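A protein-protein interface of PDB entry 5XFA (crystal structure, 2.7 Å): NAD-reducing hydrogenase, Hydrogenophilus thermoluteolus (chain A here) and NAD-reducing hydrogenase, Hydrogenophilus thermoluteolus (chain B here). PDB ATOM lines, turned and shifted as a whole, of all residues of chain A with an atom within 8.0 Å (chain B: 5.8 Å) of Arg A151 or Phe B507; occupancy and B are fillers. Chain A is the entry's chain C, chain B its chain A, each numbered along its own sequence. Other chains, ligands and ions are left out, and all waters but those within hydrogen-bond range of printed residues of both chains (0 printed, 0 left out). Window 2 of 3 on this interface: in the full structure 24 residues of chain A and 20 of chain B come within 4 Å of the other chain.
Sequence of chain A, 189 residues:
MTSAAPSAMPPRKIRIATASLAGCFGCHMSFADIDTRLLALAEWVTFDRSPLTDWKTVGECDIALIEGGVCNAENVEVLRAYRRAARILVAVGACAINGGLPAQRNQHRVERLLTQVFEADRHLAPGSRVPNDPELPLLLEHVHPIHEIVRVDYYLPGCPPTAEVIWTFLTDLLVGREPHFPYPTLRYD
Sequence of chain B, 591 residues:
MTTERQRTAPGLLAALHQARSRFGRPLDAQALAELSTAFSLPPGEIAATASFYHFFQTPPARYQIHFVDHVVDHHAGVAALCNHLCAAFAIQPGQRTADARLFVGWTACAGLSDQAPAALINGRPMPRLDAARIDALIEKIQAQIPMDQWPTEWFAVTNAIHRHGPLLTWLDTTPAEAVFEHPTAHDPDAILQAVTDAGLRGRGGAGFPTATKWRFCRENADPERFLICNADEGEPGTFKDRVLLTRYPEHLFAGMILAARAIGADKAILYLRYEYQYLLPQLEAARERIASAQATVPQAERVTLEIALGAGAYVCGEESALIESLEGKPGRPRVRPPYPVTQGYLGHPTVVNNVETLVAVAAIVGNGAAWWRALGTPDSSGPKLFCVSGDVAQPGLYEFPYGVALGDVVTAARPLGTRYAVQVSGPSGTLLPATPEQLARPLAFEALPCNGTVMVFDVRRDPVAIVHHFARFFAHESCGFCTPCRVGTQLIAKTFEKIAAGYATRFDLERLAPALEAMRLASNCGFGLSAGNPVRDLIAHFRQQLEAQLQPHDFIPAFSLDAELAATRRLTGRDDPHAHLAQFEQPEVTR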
ATOM      1  N   ILE A  66      24.683  -8.460  -6.702  1.00  0.00           N
ATOM      2  CA  ILE A  66      23.503  -8.034  -7.420  1.00  0.00           C
ATOM      3  C   ILE A  66      22.411  -9.040  -7.189  1.00  0.00           C
ATOM      4  O   ILE A  66      22.582 -10.203  -7.544  1.00  0.00           O
ATOM      5  CB  ILE A  66      23.718  -8.045  -8.948  1.00  0.00           C
ATOM      6  CG1 ILE A  66      24.991  -7.287  -9.353  1.00  0.00           C
ATOM      7  CG2 ILE A  66      22.478  -7.516  -9.670  1.00  0.00           C
ATOM      8  CD1 ILE A  66      25.099  -5.892  -8.790  1.00  0.00           C
ATOM      9  N   LEU A  79      22.989  -1.833 -13.528  1.00  0.00           N
ATOM     10  CA  LEU A  79      23.750  -3.078 -13.669  1.00  0.00           C
ATOM     11  C   LEU A  79      25.083  -2.849 -14.368  1.00  0.00           C
ATOM     12  O   LEU A  79      26.121  -3.335 -13.910  1.00  0.00           O
ATOM     13  CB  LEU A  79      22.946  -4.111 -14.450  1.00  0.00           C
ATOM     14  CG  LEU A  79      23.639  -5.458 -14.699  1.00  0.00           C
ATOM     15  CD1 LEU A  79      24.093  -6.072 -13.380  1.00  0.00           C
ATOM     16  CD2 LEU A  79      22.721  -6.407 -15.451  1.00  0.00           C
ATOM     17  N   ARG A  83      28.809  -3.116 -12.981  1.00  0.00           N
ATOM     18  CA  ARG A  83      29.761  -3.944 -13.692  1.00  0.00           C
ATOM     19  C   ARG A  83      31.099  -3.185 -13.849  1.00  0.00           C
ATOM     20  O   ARG A  83      32.125  -3.683 -13.394  1.00  0.00           O
ATOM     21  CB  ARG A  83      29.216  -4.432 -15.064  1.00  0.00           C
ATOM     22  CG  ARG A  83      29.849  -5.714 -15.606  1.00  0.00           C
ATOM     23  CD  ARG A  83      31.200  -6.010 -14.982  1.00  0.00           C
ATOM     24  NE  ARG A  83      31.432  -7.437 -14.821  1.00  0.00           N
ATOM     25  CZ  ARG A  83      32.241  -7.984 -13.914  1.00  0.00           C
ATOM     26  NH1 ARG A  83      32.390  -9.301 -13.912  1.00  0.00           N
ATOM     27  NH2 ARG A  83      32.906  -7.247 -13.012  1.00  0.00           N
ATOM     28  N   ALA A  86      33.132  -2.665 -10.558  1.00  0.00           N
ATOM     29  CA  ALA A  86      33.444  -3.798  -9.690  1.00  0.00           C
ATOM     30  C   ALA A  86      34.279  -4.863 -10.394  1.00  0.00           C
ATOM     31  O   ALA A  86      34.034  -5.196 -11.561  1.00  0.00           O
ATOM     32  CB  ALA A  86      32.161  -4.416  -9.155  1.00  0.00           C
ATOM     33  N   ARG A  87      35.255  -5.409  -9.669  1.00  0.00           N
ATOM     34  CA  ARG A  87      36.161  -6.406 -10.233  1.00  0.00           C
ATOM     35  C   ARG A  87      35.480  -7.770 -10.381  1.00  0.00           C
ATOM     36  O   ARG A  87      35.483  -8.365 -11.445  1.00  0.00           O
ATOM     37  CB  ARG A  87      37.409  -6.507  -9.357  1.00  0.00           C
ATOM     38  CG  ARG A  87      38.604  -7.165 -10.036  1.00  0.00           C
ATOM     39  CD  ARG A  87      39.874  -6.902  -9.245  1.00  0.00           C
ATOM     40  NE  ARG A  87      39.720  -7.298  -7.842  1.00  0.00           N
ATOM     41  CZ  ARG A  87      39.812  -8.550  -7.382  1.00  0.00           C
ATOM     42  NH1 ARG A  87      40.068  -9.571  -8.202  1.00  0.00           N
ATOM     43  NH2 ARG A  87      39.642  -8.787  -6.082  1.00  0.00           N
ATOM     44  N   ILE A  88      34.889  -8.228  -9.289  1.00  0.00           N
ATOM     45  CA  ILE A  88      34.094  -9.440  -9.231  1.00  0.00           C
ATOM     46  C   ILE A  88      32.613  -9.048  -9.122  1.00  0.00           C
ATOM     47  O   ILE A  88      32.222  -8.409  -8.148  1.00  0.00           O
ATOM     48  CB  ILE A  88      34.474 -10.239  -7.970  1.00  0.00           C
ATOM     49  CG1 ILE A  88      35.856 -10.851  -8.145  1.00  0.00           C
ATOM     50  CG2 ILE A  88      33.431 -11.299  -7.642  1.00  0.00           C
ATOM     51  CD1 ILE A  88      36.450 -11.381  -6.849  1.00  0.00           C
ATOM     52  N   LEU A  89      31.788  -9.411 -10.100  1.00  0.00           N
ATOM     53  CA  LEU A  89      30.343  -9.143 -10.023  1.00  0.00           C
ATOM     54  C   LEU A  89      29.621 -10.460  -9.809  1.00  0.00           C
ATOM     55  O   LEU A  89      29.858 -11.401 -10.540  1.00  0.00           O
ATOM     56  CB  LEU A  89      29.842  -8.446 -11.294  1.00  0.00           C
ATOM     57  CG  LEU A  89      28.342  -8.131 -11.293  1.00  0.00           C
ATOM     58  CD1 LEU A  89      28.024  -6.825 -12.014  1.00  0.00           C
ATOM     59  CD2 LEU A  89      27.535  -9.274 -11.889  1.00  0.00           C
ATOM     60  N   VAL A  90      28.728 -10.516  -8.832  1.00  0.00           N
ATOM     61  CA  VAL A  90      28.096 -11.767  -8.402  1.00  0.00           C
ATOM     62  C   VAL A  90      26.579 -11.712  -8.560  1.00  0.00           C
ATOM     63  O   VAL A  90      25.931 -10.801  -8.030  1.00  0.00           O
ATOM     64  CB  VAL A  90      28.419 -12.064  -6.914  1.00  0.00           C
ATOM     65  CG1 VAL A  90      27.710 -13.317  -6.436  1.00  0.00           C
ATOM     66  CG2 VAL A  90      29.915 -12.223  -6.712  1.00  0.00           C
ATOM     67  N   ALA A  91      26.029 -12.692  -9.275  1.00  0.00           N
ATOM     68  CA  ALA A  91      24.596 -12.850  -9.438  1.00  0.00           C
ATOM     69  C   ALA A  91      24.055 -13.713  -8.295  1.00  0.00           C
ATOM     70  O   ALA A  91      24.272 -14.925  -8.214  1.00  0.00           O
ATOM     71  CB  ALA A  91      24.265 -13.477 -10.778  1.00  0.00           C
ATOM     72  N   ILE A 146      20.756 -11.414 -15.197  1.00  0.00           N
ATOM     73  CA  ILE A 146      21.796 -10.402 -15.395  1.00  0.00           C
ATOM     74  C   ILE A 146      22.827 -10.822 -16.452  1.00  0.00           C
ATOM     75  O   ILE A 146      23.323  -9.967 -17.183  1.00  0.00           O
ATOM     76  CB  ILE A 146      22.507  -9.964 -14.097  1.00  0.00           C
ATOM     77  CG1 ILE A 146      23.488 -11.017 -13.629  1.00  0.00           C
ATOM     78  CG2 ILE A 146      21.508  -9.641 -12.987  1.00  0.00           C
ATOM     79  CD1 ILE A 146      24.258 -10.560 -12.421  1.00  0.00           C
ATOM     80  N   HIS A 147      23.107 -12.127 -16.577  1.00  0.00           N
ATOM     81  CA  HIS A 147      24.146 -12.609 -17.514  1.00  0.00           C
ATOM     82  C   HIS A 147      23.845 -12.353 -18.995  1.00  0.00           C
ATOM     83  O   HIS A 147      24.731 -12.418 -19.844  1.00  0.00           O
ATOM     84  CB  HIS A 147      24.570 -14.075 -17.242  1.00  0.00           C
ATOM     85  CG  HIS A 147      23.598 -15.117 -17.683  1.00  0.00           C
ATOM     86  ND1 HIS A 147      23.361 -16.255 -16.942  1.00  0.00           N
ATOM     87  CD2 HIS A 147      22.858 -15.244 -18.811  1.00  0.00           C
ATOM     88  CE1 HIS A 147      22.496 -17.024 -17.579  1.00  0.00           C
ATOM     89  NE2 HIS A 147      22.172 -16.433 -18.715  1.00  0.00           N
ATOM     90  N   GLU A 148      22.597 -12.030 -19.294  1.00  0.00           N
ATOM     91  CA  GLU A 148      22.200 -11.686 -20.650  1.00  0.00           C
ATOM     92  C   GLU A 148      22.585 -10.245 -20.993  1.00  0.00           C
ATOM     93  O   GLU A 148      22.593  -9.863 -22.154  1.00  0.00           O
ATOM     94  CB  GLU A 148      20.695 -11.893 -20.793  1.00  0.00           C
ATOM     95  CG  GLU A 148      20.279 -12.452 -22.138  1.00  0.00           C
ATOM     96  CD  GLU A 148      18.886 -13.037 -22.087  1.00  0.00           C
ATOM     97  OE1 GLU A 148      18.326 -13.087 -20.983  1.00  0.00           O
ATOM     98  OE2 GLU A 148      18.350 -13.443 -23.137  1.00  0.00           O
ATOM     99  N   ILE A 149      22.894  -9.460 -19.959  1.00  0.00           N
ATOM    100  CA  ILE A 149      23.253  -8.051 -20.086  1.00  0.00           C
ATOM    101  C   ILE A 149      24.731  -7.805 -19.811  1.00  0.00           C
ATOM    102  O   ILE A 149      25.369  -7.052 -20.534  1.00  0.00           O
ATOM    103  CB  ILE A 149      22.411  -7.207 -19.110  1.00  0.00           C
ATOM    104  CG1 ILE A 149      20.906  -7.405 -19.375  1.00  0.00           C
ATOM    105  CG2 ILE A 149      22.784  -5.731 -19.179  1.00  0.00           C
ATOM    106  CD1 ILE A 149      20.434  -7.047 -20.774  1.00  0.00           C
ATOM    107  N   VAL A 150      25.284  -8.435 -18.774  1.00  0.00           N
ATOM    108  CA  VAL A 150      26.713  -8.295 -18.460  1.00  0.00           C
ATOM    109  C   VAL A 150      27.337  -9.595 -17.955  1.00  0.00           C
ATOM    110  O   VAL A 150      26.633 -10.553 -17.636  1.00  0.00           O
ATOM    111  CB  VAL A 150      26.985  -7.213 -17.383  1.00  0.00           C
ATOM    112  CG1 VAL A 150      26.418  -5.872 -17.815  1.00  0.00           C
ATOM    113  CG2 VAL A 150      26.437  -7.648 -16.024  1.00  0.00           C
ATOM    114  N   ARG A 151      28.667  -9.597 -17.858  1.00  0.00           N
ATOM    115  CA  ARG A 151      29.386 -10.784 -17.442  1.00  0.00           C
ATOM    116  C   ARG A 151      29.335 -10.938 -15.973  1.00  0.00           C
ATOM    117  O   ARG A 151      29.441  -9.956 -15.242  1.00  0.00           O
ATOM    118  CB  ARG A 151      30.843 -10.765 -17.881  1.00  0.00           C
ATOM    119  CG  ARG A 151      31.000 -11.367 -19.249  1.00  0.00           C
ATOM    120  CD  ARG A 151      32.440 -11.407 -19.670  1.00  0.00           C
ATOM    121  NE  ARG A 151      33.153 -12.488 -19.014  1.00  0.00           N
ATOM    122  CZ  ARG A 151      34.224 -13.085 -19.523  1.00  0.00           C
ATOM    123  NH1 ARG A 151      34.721 -12.716 -20.711  1.00  0.00           N
ATOM    124  NH2 ARG A 151      34.799 -14.068 -18.843  1.00  0.00           N
ATOM    125  N   VAL A 152      29.219 -12.191 -15.557  1.00  0.00           N
ATOM    126  CA  VAL A 152      29.021 -12.557 -14.176  1.00  0.00           C
ATOM    127  C   VAL A 152      30.162 -13.453 -13.767  1.00  0.00           C
ATOM    128  O   VAL A 152      30.543 -14.336 -14.490  1.00  0.00           O
ATOM    129  CB  VAL A 152      27.685 -13.301 -14.017  1.00  0.00           C
ATOM    130  CG1 VAL A 152      27.492 -13.843 -12.600  1.00  0.00           C
ATOM    131  CG2 VAL A 152      26.548 -12.380 -14.428  1.00  0.00           C
ATOM    132  N   ASP A 153      30.720 -13.215 -12.600  1.00  0.00           N
ATOM    133  CA  ASP A 153      31.859 -13.986 -12.169  1.00  0.00           C
ATOM    134  C   ASP A 153      31.424 -15.172 -11.349  1.00  0.00           C
ATOM    135  O   ASP A 153      32.064 -16.203 -11.394  1.00  0.00           O
ATOM    136  CB  ASP A 153      32.825 -13.098 -11.392  1.00  0.00           C
ATOM    137  CG  ASP A 153      33.387 -11.973 -12.258  1.00  0.00           C
ATOM    138  OD1 ASP A 153      34.071 -12.277 -13.257  1.00  0.00           O
ATOM    139  OD2 ASP A 153      33.152 -10.790 -11.941  1.00  0.00           O
ATOM    140  N   TYR A 154      30.342 -15.035 -10.602  1.00  0.00           N
ATOM    141  CA  TYR A 154      29.850 -16.124  -9.769  1.00  0.00           C
ATOM    142  C   TYR A 154      28.337 -16.077  -9.637  1.00  0.00           C
ATOM    143  O   TYR A 154      27.730 -15.022  -9.793  1.00  0.00           O
ATOM    144  CB  TYR A 154      30.496 -16.048  -8.387  1.00  0.00           C
ATOM    145  CG  TYR A 154      31.999 -16.260  -8.382  1.00  0.00           C
ATOM    146  CD1 TYR A 154      32.531 -17.507  -8.629  1.00  0.00           C
ATOM    147  CD2 TYR A 154      32.881 -15.215  -8.117  1.00  0.00           C
ATOM    148  CE1 TYR A 154      33.888 -17.714  -8.639  1.00  0.00           C
ATOM    149  CE2 TYR A 154      34.248 -15.421  -8.108  1.00  0.00           C
ATOM    150  CZ  TYR A 154      34.740 -16.678  -8.379  1.00  0.00           C
ATOM    151  OH  TYR A 154      36.085 -16.928  -8.373  1.00  0.00           O
ATOM    152  N   TYR A 155      27.736 -17.220  -9.340  1.00  0.00           N
ATOM    153  CA  TYR A 155      26.308 -17.287  -9.076  1.00  0.00           C
ATOM    154  C   TYR A 155      26.082 -17.872  -7.678  1.00  0.00           C
ATOM    155  O   TYR A 155      26.729 -18.846  -7.300  1.00  0.00           O
ATOM    156  CB  TYR A 155      25.619 -18.186 -10.115  1.00  0.00           C
ATOM    157  CG  TYR A 155      25.835 -17.807 -11.569  1.00  0.00           C
ATOM    158  CD1 TYR A 155      26.881 -18.335 -12.309  1.00  0.00           C
ATOM    159  CD2 TYR A 155      24.993 -16.906 -12.198  1.00  0.00           C
ATOM    160  CE1 TYR A 155      27.075 -17.986 -13.638  1.00  0.00           C
ATOM    161  CE2 TYR A 155      25.174 -16.554 -13.520  1.00  0.00           C
ATOM    162  CZ  TYR A 155      26.214 -17.095 -14.234  1.00  0.00           C
ATOM    163  OH  TYR A 155      26.362 -16.733 -15.545  1.00  0.00           O
ATOM    164  N   THR B 505      31.220 -11.520 -29.004  1.00  0.00           N
ATOM    165  CA  THR B 505      32.554 -11.265 -28.437  1.00  0.00           C
ATOM    166  C   THR B 505      33.255 -12.592 -28.160  1.00  0.00           C
ATOM    167  O   THR B 505      32.696 -13.643 -28.414  1.00  0.00           O
ATOM    168  CB  THR B 505      32.473 -10.428 -27.131  1.00  0.00           C
ATOM    169  OG1 THR B 505      32.080 -11.260 -26.037  1.00  0.00           O
ATOM    170  CG2 THR B 505      31.477  -9.288 -27.262  1.00  0.00           C
ATOM    171  N   ARG B 506      34.469 -12.547 -27.626  1.00  0.00           N
ATOM    172  CA  ARG B 506      35.214 -13.768 -27.307  1.00  0.00           C
ATOM    173  C   ARG B 506      34.450 -14.669 -26.343  1.00  0.00           C
ATOM    174  O   ARG B 506      34.448 -15.898 -26.489  1.00  0.00           O
ATOM    175  CB  ARG B 506      36.561 -13.435 -26.673  1.00  0.00           C
ATOM    176  CG  ARG B 506      37.544 -14.604 -26.683  1.00  0.00           C
ATOM    177  CD  ARG B 506      38.944 -14.147 -27.069  1.00  0.00           C
ATOM    178  NE  ARG B 506      38.911 -13.257 -28.233  1.00  0.00           N
ATOM    179  CZ  ARG B 506      39.974 -12.666 -28.771  1.00  0.00           C
ATOM    180  NH1 ARG B 506      41.191 -12.877 -28.278  1.00  0.00           N
ATOM    181  NH2 ARG B 506      39.812 -11.872 -29.824  1.00  0.00           N
ATOM    182  N   PHE B 507      33.807 -14.048 -25.359  1.00  0.00           N
ATOM    183  CA  PHE B 507      33.054 -14.782 -24.354  1.00  0.00           C
ATOM    184  C   PHE B 507      31.955 -15.661 -24.945  1.00  0.00           C
ATOM    185  O   PHE B 507      31.592 -16.658 -24.352  1.00  0.00           O
ATOM    186  CB  PHE B 507      32.434 -13.815 -23.332  1.00  0.00           C
ATOM    187  CG  PHE B 507      31.655 -14.512 -22.264  1.00  0.00           C
ATOM    188  CD1 PHE B 507      32.317 -15.236 -21.275  1.00  0.00           C
ATOM    189  CD2 PHE B 507      30.267 -14.503 -22.278  1.00  0.00           C
ATOM    190  CE1 PHE B 507      31.606 -15.909 -20.293  1.00  0.00           C
ATOM    191  CE2 PHE B 507      29.553 -15.180 -21.307  1.00  0.00           C
ATOM    192  CZ  PHE B 507      30.220 -15.880 -20.311  1.00  0.00           C
ATOM    193  N   ASP B 508      31.399 -15.273 -26.086  1.00  0.00           N
ATOM    194  CA  ASP B 508      30.294 -16.020 -26.683  1.00  0.00           C
ATOM    195  C   ASP B 508      30.747 -17.380 -27.234  1.00  0.00           C
ATOM    196  O   ASP B 508      29.958 -18.319 -27.270  1.00  0.00           O
ATOM    197  CB  ASP B 508      29.609 -15.183 -27.776  1.00  0.00           C
ATOM    198  CG  ASP B 508      28.967 -13.894 -27.224  1.00  0.00           C
ATOM    199  OD1 ASP B 508      28.076 -13.991 -26.369  1.00  0.00           O
ATOM    200  OD2 ASP B 508      29.345 -12.776 -27.647  1.00  0.00           O
ATOM    201  N   LEU B 509      32.014 -17.484 -27.634  1.00  0.00           N
ATOM    202  CA  LEU B 509      32.571 -18.747 -28.117  1.00  0.00           C
ATOM    203  C   LEU B 509      33.054 -19.615 -26.986  1.00  0.00           C
ATOM    204  O   LEU B 509      33.176 -20.817 -27.122  1.00  0.00           O
ATOM    205  CB  LEU B 509      33.725 -18.507 -29.080  1.00  0.00           C
ATOM    206  CG  LEU B 509      33.336 -18.289 -30.540  1.00  0.00           C
ATOM    207  CD1 LEU B 509      32.181 -17.313 -30.671  1.00  0.00           C
ATOM    208  CD2 LEU B 509      34.544 -17.788 -31.310  1.00  0.00           C
ATOM    209  N   GLU B 510      33.353 -19.001 -25.871  1.00  0.00           N
ATOM    210  CA  GLU B 510      33.784 -19.720 -24.708  1.00  0.00           C
ATOM    211  C   GLU B 510      32.601 -20.411 -24.031  1.00  0.00           C
ATOM    212  O   GLU B 510      32.765 -21.466 -23.416  1.00  0.00           O
ATOM    213  CB  GLU B 510      34.360 -18.692 -23.739  1.00  0.00           C
ATOM    214  CG  GLU B 510      35.632 -19.062 -23.014  1.00  0.00           C
ATOM    215  CD  GLU B 510      36.060 -17.967 -22.048  1.00  0.00           C
ATOM    216  OE1 GLU B 510      36.707 -18.307 -21.033  1.00  0.00           O
ATOM    217  OE2 GLU B 510      35.747 -16.770 -22.308  1.00  0.00           O
ATOM    218  N   ARG B 511      31.430 -19.779 -24.069  1.00  0.00           N
ATOM    219  CA  ARG B 511      30.227 -20.356 -23.467  1.00  0.00           C
ATOM    220  C   ARG B 511      29.637 -21.409 -24.398  1.00  0.00           C
ATOM    221  O   ARG B 511      28.928 -22.305 -23.953  1.00  0.00           O
ATOM    222  CB  ARG B 511      29.186 -19.280 -23.102  1.00  0.00           C
ATOM    223  CG  ARG B 511      28.097 -19.035 -24.143  1.00  0.00           C
ATOM    224  CD  ARG B 511      27.354 -17.733 -23.915  1.00  0.00           C
ATOM    225  NE  ARG B 511      26.469 -17.771 -22.750  1.00  0.00           N
ATOM    226  CZ  ARG B 511      25.578 -16.824 -22.457  1.00  0.00           C
ATOM    227  NH1 ARG B 511      25.447 -15.745 -23.219  1.00  0.00           N
ATOM    228  NH2 ARG B 511      24.810 -16.955 -21.386  1.00  0.00           N
ATOM    229  N   LEU B 512      29.928 -21.295 -25.689  1.00  0.00           N
ATOM    230  CA  LEU B 512      29.399 -22.237 -26.661  1.00  0.00           C
ATOM    231  C   LEU B 512      30.168 -23.555 -26.703  1.00  0.00           C
ATOM    232  O   LEU B 512      29.612 -24.579 -27.094  1.00  0.00           O
ATOM    233  CB  LEU B 512      29.381 -21.616 -28.053  1.00  0.00           C
ATOM    234  CG  LEU B 512      28.769 -22.504 -29.144  1.00  0.00           C
ATOM    235  CD1 LEU B 512      27.384 -22.985 -28.737  1.00  0.00           C
ATOM    236  CD2 LEU B 512      28.717 -21.774 -30.484  1.00  0.00           C
ATOM    237  N   ASP B 554      34.031  -7.089 -23.638  1.00  0.00           N
ATOM    238  CA  ASP B 554      33.982  -8.304 -22.790  1.00  0.00           C
ATOM    239  C   ASP B 554      32.649  -9.052 -22.862  1.00  0.00           C
ATOM    240  O   ASP B 554      32.608 -10.268 -22.649  1.00  0.00           O
ATOM    241  CB  ASP B 554      34.240  -7.967 -21.315  1.00  0.00           C
ATOM    242  CG  ASP B 554      35.586  -7.321 -21.079  1.00  0.00           C
ATOM    243  OD1 ASP B 554      36.412  -7.251 -22.020  1.00  0.00           O
ATOM    244  OD2 ASP B 554      35.815  -6.883 -19.934  1.00  0.00           O
ATOM    245  N   PHE B 555      31.571  -8.312 -23.108  1.00  0.00           N
ATOM    246  CA  PHE B 555      30.248  -8.884 -23.362  1.00  0.00           C
ATOM    247  C   PHE B 555      29.303  -7.841 -23.951  1.00  0.00           C
ATOM    248  O   PHE B 555      29.405  -6.677 -23.629  1.00  0.00           O
ATOM    249  CB  PHE B 555      29.628  -9.460 -22.079  1.00  0.00           C
ATOM    250  CG  PHE B 555      28.283 -10.095 -22.301  1.00  0.00           C
ATOM    251  CD1 PHE B 555      27.122  -9.396 -22.045  1.00  0.00           C
ATOM    252  CD2 PHE B 555      28.188 -11.372 -22.823  1.00  0.00           C
ATOM    253  CE1 PHE B 555      25.878  -9.960 -22.274  1.00  0.00           C
ATOM    254  CE2 PHE B 555      26.954 -11.941 -23.063  1.00  0.00           C
ATOM    255  CZ  PHE B 555      25.795 -11.234 -22.781  1.00  0.00           C
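The backbone NH (N) of Phe B507 sits close to the side-chain hydroxyl (OG1) of Thr B505 (3.3 Å).
The backbone carbonyl oxygen of Arg A151 is in hydrogen-bond range of the guanidinium group of Arg A83, 3.2 Å away.
ND1 of His A147 sits at hydrogen-bond distance from OH of Tyr A155 (3.3 Å).
NH2 of Arg B511 touches CD2 of His A147 (3.7 Å).
His A147 touches Phe B555.
Phe B555 touches Glu A148.
Ile A149 touches Phe B555 (O to CD1, 3.3 Å).
Val A150 touches Phe B555 (CA to CD1, 3.8 Å).
Phe B507 touches Arg A151 (CD1 to CZ, 3.4 Å).
Asp B554 touches Arg A151 (O to CD, 3.2 Å).
Phe B555 touches Arg A151.
Printed residues of chain B within 4 Å of Arg A151: Phe B507, Asp B554 and Phe B555.
Phe B507 touches just one residue of chain A: Arg A151 (3.4 Å).
Printed residues of chain B within 4 Å of His A147: Arg B511 (3.7 Å) and Phe B555 (3.3 Å).
Printed residues of chain A within 4 Å of Phe B555: His A147 (3.3 Å), Glu A148 (3.3 Å), Ile A149 (3.3 Å), Val A150 (3.8 Å) and Arg A151 (3.7 Å).
Leu B512 touches none of the printed residues of chain A.
Ala A86 touches none of the printed residues of chain B.
The nearest printed residue of chain A that does not touch Asp B554 is Arg A83 (6.8 Å).
Of the 19 printed residues of chain A, 5 touch a printed residue of chain B.
Printed residues of chain A that touch a printed residue of chain B: His A147, Glu A148, Ile A149, Val A150 and Arg A151.
Of the 10 printed residues of chain B, 4 touch a printed residue of chain A.
Printed residues of chain B that touch a printed residue of chain A: Phe B507, Arg B511, Asp B554 and Phe B555.
Hydrophobic or aromatic side chains of chain B that line the printed part of chain A: Phe B507 and Phe B555.
Among the printed residues, no Asp or Glu carboxylate lies within 4 Å of a Lys or Arg side-chain nitrogen of the other chain.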
